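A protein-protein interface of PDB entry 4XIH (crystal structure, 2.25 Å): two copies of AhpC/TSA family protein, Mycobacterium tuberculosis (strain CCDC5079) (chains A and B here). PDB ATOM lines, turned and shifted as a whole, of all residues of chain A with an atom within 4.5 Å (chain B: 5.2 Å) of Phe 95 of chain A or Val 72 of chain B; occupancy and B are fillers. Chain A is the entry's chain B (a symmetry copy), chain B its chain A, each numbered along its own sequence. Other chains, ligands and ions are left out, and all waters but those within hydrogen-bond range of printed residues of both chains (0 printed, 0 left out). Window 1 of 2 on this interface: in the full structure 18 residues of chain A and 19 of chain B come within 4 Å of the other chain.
The backbone NH (N) of Phe 108 of chain B is in hydrogen-bond range of the backbone carbonyl oxygen (O) of Ser 102 of chain B, at 3.5 Å.
A ring nitrogen (NE2) of His 98 of chain B sits at hydrogen-bond distance from the backbone carbonyl oxygen (O) of Gly 113 of chain B, 2.6 Å away.
ND1 of His 98 of chain A is in hydrogen-bond range of ND1 of His 98 of chain B.
The indole nitrogen of Trp 96 of chain A lies close to the backbone NH of Gly 113 of chain B, 3.5 Å away.
Val 72 of chain A touches Phe 95 of chain B, and with the chains exchanged Phe 95 of chain A touches Val 72 of chain B.
Phe 95 of chain A touches His 98 of chain B, and with the chains exchanged His 98 of chain A touches Phe 95 of chain B.
His 98 of chain B touches its own counterpart, His 98 of chain A.
Of the 13 pairs that touch across the chains among the printed residues, 5 have their exchanged pair printed and touching as well.
Of the 9 printed residues of chain A, 5 touch a printed residue of chain B.
Hydrophobic or aromatic side chains of chain A within 4 Å of the printed part of chain B: Val 72, Pro 74, Phe 95, Trp 96 and His 98.
Among the printed residues, no Asp or Glu carboxylate lies within 4 Å of a Lys or Arg side-chain nitrogen of the other chain.
Phe 95 of chain A touches just these residues of chain B: Val 72, His 98, Ala 112, Gly 113 and Ile 114.
Val 72 of chain B touches just one residue of chain A: Phe 95 (3.6 Å).
Printed residues of chain A within 4 Å of His 98 of chain B: Phe 95, Trp 96 and His 98.
Printed residues of chain B within 4 Å of Pro 74 of chain A: Leu 40 (3.6 Å).
Of the printed residues of chain B, Trp 96 of chain A touches His 98, Phe 108, Ala 112 and Gly 113.
Of the printed residues of chain A, Gly 113 of chain B touches Phe 95 (3.4 Å) and Trp 96 (3.4 Å).
The nearest printed residue of chain B that does not touch Val 72 of chain A is His 98 of chain B (6.2 Å).
Among the printed residues, merely in contact across the chains: Trp 96 of chain A with His 98 of chain B, Phe 95 of chain A with Gly 113 of chain B, Phe 95 of chain A with Ala 112 of chain B, Trp 96 of chain A with Ala 112 of chain B, Phe 95 of chain A with Val 72 of chain B, Pro 74 of chain A with Leu 40 of chain B, Val 72 of chain A with Phe 95 of chain B, Phe 95 of chain A with Ile 114 of chain B, His 98 of chain A with Phe 95 of chain B, Phe 95 of chain A with His 98 of chain B and Trp 96 of chain A with Phe 108 of chain B.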
ATOM      1  N   VAL A  72      32.100   9.915 -24.712  1.00  0.00           N
ATOM      2  CA  VAL A  72      30.831   9.241 -24.979  1.00  0.00           C
ATOM      3  C   VAL A  72      29.696   9.641 -24.034  1.00  0.00           C
ATOM      4  O   VAL A  72      28.558   9.213 -24.229  1.00  0.00           O
ATOM      5  CB  VAL A  72      30.984   7.705 -24.985  1.00  0.00           C
ATOM      6  CG1 VAL A  72      32.032   7.288 -26.010  1.00  0.00           C
ATOM      7  CG2 VAL A  72      31.323   7.170 -23.598  1.00  0.00           C
ATOM      8  N   GLY A  73      29.995  10.458 -23.026  1.00  0.00           N
ATOM      9  CA  GLY A  73      28.983  10.906 -22.083  1.00  0.00           C
ATOM     10  C   GLY A  73      27.982  11.880 -22.685  1.00  0.00           C
ATOM     11  O   GLY A  73      28.320  12.633 -23.595  1.00  0.00           O
ATOM     12  N   PRO A  74      26.736  11.865 -22.185  1.00  0.00           N
ATOM     13  CA  PRO A  74      25.710  12.782 -22.679  1.00  0.00           C
ATOM     14  C   PRO A  74      25.831  14.158 -22.020  1.00  0.00           C
ATOM     15  O   PRO A  74      26.525  14.288 -21.016  1.00  0.00           O
ATOM     16  CB  PRO A  74      24.410  12.086 -22.284  1.00  0.00           C
ATOM     17  CG  PRO A  74      24.760  11.334 -21.049  1.00  0.00           C
ATOM     18  CD  PRO A  74      26.187  10.901 -21.214  1.00  0.00           C
ATOM     19  N   SER A  93      29.350  15.556 -26.708  1.00  0.00           N
ATOM     20  CA  SER A  93      28.808  14.230 -26.428  1.00  0.00           C
ATOM     21  C   SER A  93      28.781  13.311 -27.635  1.00  0.00           C
ATOM     22  O   SER A  93      27.963  13.479 -28.541  1.00  0.00           O
ATOM     23  CB  SER A  93      27.396  14.362 -25.863  1.00  0.00           C
ATOM     24  OG  SER A  93      27.430  15.022 -24.608  1.00  0.00           O
ATOM     25  N   ASP A  94      29.670  12.326 -27.625  1.00  0.00           N
ATOM     26  CA  ASP A  94      29.748  11.308 -28.664  1.00  0.00           C
ATOM     27  C   ASP A  94      28.916  10.137 -28.123  1.00  0.00           C
ATOM     28  O   ASP A  94      29.365   8.995 -28.051  1.00  0.00           O
ATOM     29  CB  ASP A  94      31.217  10.930 -28.856  1.00  0.00           C
ATOM     30  CG  ASP A  94      31.473  10.173 -30.134  1.00  0.00           C
ATOM     31  OD1 ASP A  94      30.615  10.195 -31.042  1.00  0.00           O
ATOM     32  OD2 ASP A  94      32.567   9.581 -30.245  1.00  0.00           O
ATOM     33  N   PHE A  95      27.669  10.456 -27.781  1.00  0.00           N
ATOM     34  CA  PHE A  95      26.762   9.562 -27.069  1.00  0.00           C
ATOM     35  C   PHE A  95      25.894   8.640 -27.918  1.00  0.00           C
ATOM     36  O   PHE A  95      25.747   7.461 -27.590  1.00  0.00           O
ATOM     37  CB  PHE A  95      25.868  10.429 -26.176  1.00  0.00           C
ATOM     38  CG  PHE A  95      24.859   9.658 -25.381  1.00  0.00           C
ATOM     39  CD1 PHE A  95      25.235   8.985 -24.229  1.00  0.00           C
ATOM     40  CD2 PHE A  95      23.525   9.638 -25.763  1.00  0.00           C
ATOM     41  CE1 PHE A  95      24.304   8.285 -23.486  1.00  0.00           C
ATOM     42  CE2 PHE A  95      22.590   8.939 -25.024  1.00  0.00           C
ATOM     43  CZ  PHE A  95      22.982   8.263 -23.883  1.00  0.00           C
ATOM     44  N   TRP A  96      25.306   9.169 -28.985  1.00  0.00           N
ATOM     45  CA  TRP A  96      24.413   8.368 -29.825  1.00  0.00           C
ATOM     46  C   TRP A  96      24.388   8.892 -31.267  1.00  0.00           C
ATOM     47  O   TRP A  96      23.887   9.991 -31.503  1.00  0.00           O
ATOM     48  CB  TRP A  96      23.008   8.378 -29.222  1.00  0.00           C
ATOM     49  CG  TRP A  96      22.090   7.354 -29.804  1.00  0.00           C
ATOM     50  CD1 TRP A  96      20.955   7.584 -30.519  1.00  0.00           C
ATOM     51  CD2 TRP A  96      22.237   5.932 -29.729  1.00  0.00           C
ATOM     52  NE1 TRP A  96      20.375   6.394 -30.884  1.00  0.00           N
ATOM     53  CE2 TRP A  96      21.143   5.364 -30.413  1.00  0.00           C
ATOM     54  CE3 TRP A  96      23.184   5.083 -29.143  1.00  0.00           C
ATOM     55  CZ2 TRP A  96      20.970   3.982 -30.534  1.00  0.00           C
ATOM     56  CZ3 TRP A  96      23.014   3.707 -29.265  1.00  0.00           C
ATOM     57  CH2 TRP A  96      21.915   3.172 -29.954  1.00  0.00           C
ATOM     58  N   PRO A  97      24.909   8.125 -32.230  1.00  0.00           N
ATOM     59  CA  PRO A  97      25.497   6.792 -32.012  1.00  0.00           C
ATOM     60  C   PRO A  97      26.705   6.792 -31.069  1.00  0.00           C
ATOM     61  O   PRO A  97      27.520   7.717 -31.090  1.00  0.00           O
ATOM     62  CB  PRO A  97      25.894   6.324 -33.422  1.00  0.00           C
ATOM     63  CG  PRO A  97      25.705   7.491 -34.330  1.00  0.00           C
ATOM     64  CD  PRO A  97      24.789   8.466 -33.657  1.00  0.00           C
ATOM     65  N   HIS A  98      26.795   5.742 -30.255  1.00  0.00           N
ATOM     66  CA  HIS A  98      27.815   5.618 -29.218  1.00  0.00           C
ATOM     67  C   HIS A  98      29.246   5.556 -29.740  1.00  0.00           C
ATOM     68  O   HIS A  98      29.666   4.546 -30.303  1.00  0.00           O
ATOM     69  CB  HIS A  98      27.534   4.378 -28.365  1.00  0.00           C
ATOM     70  CG  HIS A  98      28.456   4.229 -27.200  1.00  0.00           C
ATOM     71  ND1 HIS A  98      28.101   4.588 -25.920  1.00  0.00           N
ATOM     72  CD2 HIS A  98      29.731   3.782 -27.123  1.00  0.00           C
ATOM     73  CE1 HIS A  98      29.107   4.355 -25.101  1.00  0.00           C
ATOM     74  NE2 HIS A  98      30.111   3.868 -25.806  1.00  0.00           N
ATOM     75  N   PHE B  38      15.493   4.252 -16.278  1.00  0.00           N
ATOM     76  CA  PHE B  38      15.391   5.711 -16.363  1.00  0.00           C
ATOM     77  C   PHE B  38      16.331   6.223 -17.449  1.00  0.00           C
ATOM     78  O   PHE B  38      17.367   5.615 -17.698  1.00  0.00           O
ATOM     79  CB  PHE B  38      15.666   6.377 -15.012  1.00  0.00           C
ATOM     80  CG  PHE B  38      17.070   6.208 -14.515  1.00  0.00           C
ATOM     81  CD1 PHE B  38      17.453   5.050 -13.856  1.00  0.00           C
ATOM     82  CD2 PHE B  38      18.005   7.230 -14.673  1.00  0.00           C
ATOM     83  CE1 PHE B  38      18.747   4.897 -13.384  1.00  0.00           C
ATOM     84  CE2 PHE B  38      19.298   7.083 -14.204  1.00  0.00           C
ATOM     85  CZ  PHE B  38      19.668   5.915 -13.556  1.00  0.00           C
ATOM     86  N   PRO B  39      15.959   7.331 -18.114  1.00  0.00           N
ATOM     87  CA  PRO B  39      16.762   7.840 -19.236  1.00  0.00           C
ATOM     88  C   PRO B  39      18.188   8.313 -18.936  1.00  0.00           C
ATOM     89  O   PRO B  39      19.138   7.746 -19.476  1.00  0.00           O
ATOM     90  CB  PRO B  39      15.922   8.998 -19.807  1.00  0.00           C
ATOM     91  CG  PRO B  39      14.668   9.067 -19.017  1.00  0.00           C
ATOM     92  CD  PRO B  39      14.610   7.921 -18.061  1.00  0.00           C
ATOM     93  N   LEU B  40      18.342   9.338 -18.106  1.00  0.00           N
ATOM     94  CA  LEU B  40      19.663   9.908 -17.855  1.00  0.00           C
ATOM     95  C   LEU B  40      19.840  10.457 -16.456  1.00  0.00           C
ATOM     96  O   LEU B  40      18.938  11.090 -15.905  1.00  0.00           O
ATOM     97  CB  LEU B  40      19.914  11.058 -18.838  1.00  0.00           C
ATOM     98  CG  LEU B  40      20.129  10.717 -20.313  1.00  0.00           C
ATOM     99  CD1 LEU B  40      20.080  11.974 -21.168  1.00  0.00           C
ATOM    100  CD2 LEU B  40      21.448   9.983 -20.495  1.00  0.00           C
ATOM    101  N   ILE B  70      18.078   1.255 -13.488  1.00  0.00           N
ATOM    102  CA  ILE B  70      18.938   0.964 -14.633  1.00  0.00           C
ATOM    103  C   ILE B  70      18.897   2.074 -15.683  1.00  0.00           C
ATOM    104  O   ILE B  70      17.830   2.601 -15.997  1.00  0.00           O
ATOM    105  CB  ILE B  70      18.518  -0.365 -15.309  1.00  0.00           C
ATOM    106  CG1 ILE B  70      18.440  -1.498 -14.274  1.00  0.00           C
ATOM    107  CG2 ILE B  70      19.477  -0.722 -16.439  1.00  0.00           C
ATOM    108  CD1 ILE B  70      17.975  -2.824 -14.832  1.00  0.00           C
ATOM    109  N   SER B  71      20.068   2.430 -16.208  1.00  0.00           N
ATOM    110  CA  SER B  71      20.181   3.410 -17.291  1.00  0.00           C
ATOM    111  C   SER B  71      21.467   3.152 -18.065  1.00  0.00           C
ATOM    112  O   SER B  71      22.291   2.333 -17.655  1.00  0.00           O
ATOM    113  CB  SER B  71      20.169   4.849 -16.775  1.00  0.00           C
ATOM    114  OG  SER B  71      21.394   5.187 -16.151  1.00  0.00           O
ATOM    115  N   VAL B  72      21.643   3.868 -19.170  1.00  0.00           N
ATOM    116  CA  VAL B  72      22.820   3.685 -20.028  1.00  0.00           C
ATOM    117  C   VAL B  72      24.114   4.346 -19.528  1.00  0.00           C
ATOM    118  O   VAL B  72      25.172   4.137 -20.119  1.00  0.00           O
ATOM    119  CB  VAL B  72      22.540   4.126 -21.484  1.00  0.00           C
ATOM    120  CG1 VAL B  72      21.380   3.330 -22.062  1.00  0.00           C
ATOM    121  CG2 VAL B  72      22.265   5.622 -21.577  1.00  0.00           C
ATOM    122  N   GLY B  73      24.045   5.127 -18.452  1.00  0.00           N
ATOM    123  CA  GLY B  73      25.234   5.782 -17.906  1.00  0.00           C
ATOM    124  C   GLY B  73      26.208   4.813 -17.243  1.00  0.00           C
ATOM    125  O   GLY B  73      25.799   3.756 -16.758  1.00  0.00           O
ATOM    126  N   PRO B  74      27.510   5.160 -17.225  1.00  0.00           N
ATOM    127  CA  PRO B  74      28.511   4.310 -16.589  1.00  0.00           C
ATOM    128  C   PRO B  74      28.544   4.505 -15.064  1.00  0.00           C
ATOM    129  O   PRO B  74      27.995   5.481 -14.563  1.00  0.00           O
ATOM    130  CB  PRO B  74      29.816   4.775 -17.235  1.00  0.00           C
ATOM    131  CG  PRO B  74      29.584   6.218 -17.507  1.00  0.00           C
ATOM    132  CD  PRO B  74      28.122   6.349 -17.842  1.00  0.00           C
ATOM    133  N   HIS B  78      26.836   7.326 -12.151  1.00  0.00           N
ATOM    134  CA  HIS B  78      25.845   6.937 -11.152  1.00  0.00           C
ATOM    135  C   HIS B  78      26.365   7.112  -9.740  1.00  0.00           C
ATOM    136  O   HIS B  78      25.597   7.428  -8.836  1.00  0.00           O
ATOM    137  CB  HIS B  78      25.396   5.488 -11.323  1.00  0.00           C
ATOM    138  CG  HIS B  78      24.634   5.236 -12.580  1.00  0.00           C
ATOM    139  ND1 HIS B  78      24.768   4.076 -13.310  1.00  0.00           N
ATOM    140  CD2 HIS B  78      23.745   6.004 -13.252  1.00  0.00           C
ATOM    141  CE1 HIS B  78      23.973   4.129 -14.363  1.00  0.00           C
ATOM    142  NE2 HIS B  78      23.346   5.292 -14.355  1.00  0.00           N
ATOM    143  N   ASP B  94      23.813   0.059 -18.006  1.00  0.00           N
ATOM    144  CA  ASP B  94      23.481  -0.629 -19.250  1.00  0.00           C
ATOM    145  C   ASP B  94      24.279   0.141 -20.308  1.00  0.00           C
ATOM    146  O   ASP B  94      23.746   0.561 -21.338  1.00  0.00           O
ATOM    147  CB  ASP B  94      21.967  -0.509 -19.467  1.00  0.00           C
ATOM    148  CG  ASP B  94      21.457  -1.327 -20.637  1.00  0.00           C
ATOM    149  OD1 ASP B  94      22.200  -2.176 -21.171  1.00  0.00           O
ATOM    150  OD2 ASP B  94      20.278  -1.128 -21.009  1.00  0.00           O
ATOM    151  N   PHE B  95      25.578   0.281 -20.042  1.00  0.00           N
ATOM    152  CA  PHE B  95      26.482   1.149 -20.805  1.00  0.00           C
ATOM    153  C   PHE B  95      27.135   0.557 -22.050  1.00  0.00           C
ATOM    154  O   PHE B  95      27.191   1.219 -23.089  1.00  0.00           O
ATOM    155  CB  PHE B  95      27.566   1.665 -19.847  1.00  0.00           C
ATOM    156  CG  PHE B  95      28.614   2.524 -20.500  1.00  0.00           C
ATOM    157  CD1 PHE B  95      28.350   3.850 -20.814  1.00  0.00           C
ATOM    158  CD2 PHE B  95      29.878   2.015 -20.770  1.00  0.00           C
ATOM    159  CE1 PHE B  95      29.318   4.647 -21.402  1.00  0.00           C
ATOM    160  CE2 PHE B  95      30.849   2.808 -21.360  1.00  0.00           C
ATOM    161  CZ  PHE B  95      30.568   4.125 -21.676  1.00  0.00           C
ATOM    162  N   HIS B  98      25.619  -0.662 -25.482  1.00  0.00           N
ATOM    163  CA  HIS B  98      24.746   0.467 -25.190  1.00  0.00           C
ATOM    164  C   HIS B  98      23.259   0.132 -25.241  1.00  0.00           C
ATOM    165  O   HIS B  98      22.702  -0.091 -26.317  1.00  0.00           O
ATOM    166  CB  HIS B  98      25.040   1.602 -26.170  1.00  0.00           C
ATOM    167  CG  HIS B  98      24.337   2.881 -25.848  1.00  0.00           C
ATOM    168  ND1 HIS B  98      24.990   3.971 -25.318  1.00  0.00           N
ATOM    169  CD2 HIS B  98      23.040   3.246 -25.972  1.00  0.00           C
ATOM    170  CE1 HIS B  98      24.131   4.958 -25.142  1.00  0.00           C
ATOM    171  NE2 HIS B  98      22.938   4.541 -25.526  1.00  0.00           N
ATOM    172  N   GLY B  99      22.628   0.116 -24.070  1.00  0.00           N
ATOM    173  CA  GLY B  99      21.199  -0.134 -23.956  1.00  0.00           C
ATOM    174  C   GLY B  99      20.735  -1.553 -24.235  1.00  0.00           C
ATOM    175  O   GLY B  99      19.549  -1.768 -24.463  1.00  0.00           O
ATOM    176  N   SER B 102      18.107  -2.701 -21.795  1.00  0.00           N
ATOM    177  CA  SER B 102      16.928  -1.889 -22.077  1.00  0.00           C
ATOM    178  C   SER B 102      16.208  -2.349 -23.346  1.00  0.00           C
ATOM    179  O   SER B 102      14.978  -2.363 -23.387  1.00  0.00           O
ATOM    180  CB  SER B 102      17.315  -0.416 -22.198  1.00  0.00           C
ATOM    181  OG  SER B 102      17.873   0.055 -20.984  1.00  0.00           O
ATOM    182  N   PHE B 108      13.891   0.667 -24.751  1.00  0.00           N
ATOM    183  CA  PHE B 108      14.976   1.491 -25.259  1.00  0.00           C
ATOM    184  C   PHE B 108      14.484   2.451 -26.336  1.00  0.00           C
ATOM    185  O   PHE B 108      13.756   2.059 -27.242  1.00  0.00           O
ATOM    186  CB  PHE B 108      16.093   0.609 -25.806  1.00  0.00           C
ATOM    187  CG  PHE B 108      17.302   1.376 -26.254  1.00  0.00           C
ATOM    188  CD1 PHE B 108      18.168   1.925 -25.322  1.00  0.00           C
ATOM    189  CD2 PHE B 108      17.586   1.533 -27.605  1.00  0.00           C
ATOM    190  CE1 PHE B 108      19.288   2.628 -25.725  1.00  0.00           C
ATOM    191  CE2 PHE B 108      18.707   2.233 -28.016  1.00  0.00           C
ATOM    192  CZ  PHE B 108      19.561   2.780 -27.073  1.00  0.00           C
ATOM    193  N   ALA B 112      16.986   8.729 -29.316  1.00  0.00           N
ATOM    194  CA  ALA B 112      17.861   9.427 -28.373  1.00  0.00           C
ATOM    195  C   ALA B 112      18.946   8.552 -27.732  1.00  0.00           C
ATOM    196  O   ALA B 112      19.849   9.075 -27.084  1.00  0.00           O
ATOM    197  CB  ALA B 112      17.020  10.090 -27.292  1.00  0.00           C
ATOM    198  N   GLY B 113      18.855   7.235 -27.899  1.00  0.00           N
ATOM    199  CA  GLY B 113      19.846   6.315 -27.339  1.00  0.00           C
ATOM    200  C   GLY B 113      19.808   6.187 -25.827  1.00  0.00           C
ATOM    201  O   GLY B 113      20.842   5.996 -25.186  1.00  0.00           O
ATOM    202  N   ILE B 114      18.613   6.287 -25.258  1.00  0.00           N
ATOM    203  CA  ILE B 114      18.423   6.193 -23.817  1.00  0.00           C
ATOM    204  C   ILE B 114      17.265   5.253 -23.532  1.00  0.00           C
ATOM    205  O   ILE B 114      16.483   4.935 -24.425  1.00  0.00           O
ATOM    206  CB  ILE B 114      18.128   7.577 -23.189  1.00  0.00           C
ATOM    207  CG1 ILE B 114      16.867   8.201 -23.808  1.00  0.00           C
ATOM    208  CG2 ILE B 114      19.325   8.500 -23.365  1.00  0.00           C
ATOM    209  CD1 ILE B 114      16.584   9.617 -23.359  1.00  0.00           C
ATOM    210  N   ALA B 115      17.165   4.803 -22.290  1.00  0.00           N
ATOM    211  CA  ALA B 115      16.073   3.935 -21.894  1.00  0.00           C
ATOM    212  C   ALA B 115      14.853   4.787 -21.571  1.00  0.00           C
ATOM    213  O   ALA B 115      14.977   5.857 -20.969  1.00  0.00           O
ATOM    214  CB  ALA B 115      16.470   3.107 -20.684  1.00  0.00           C
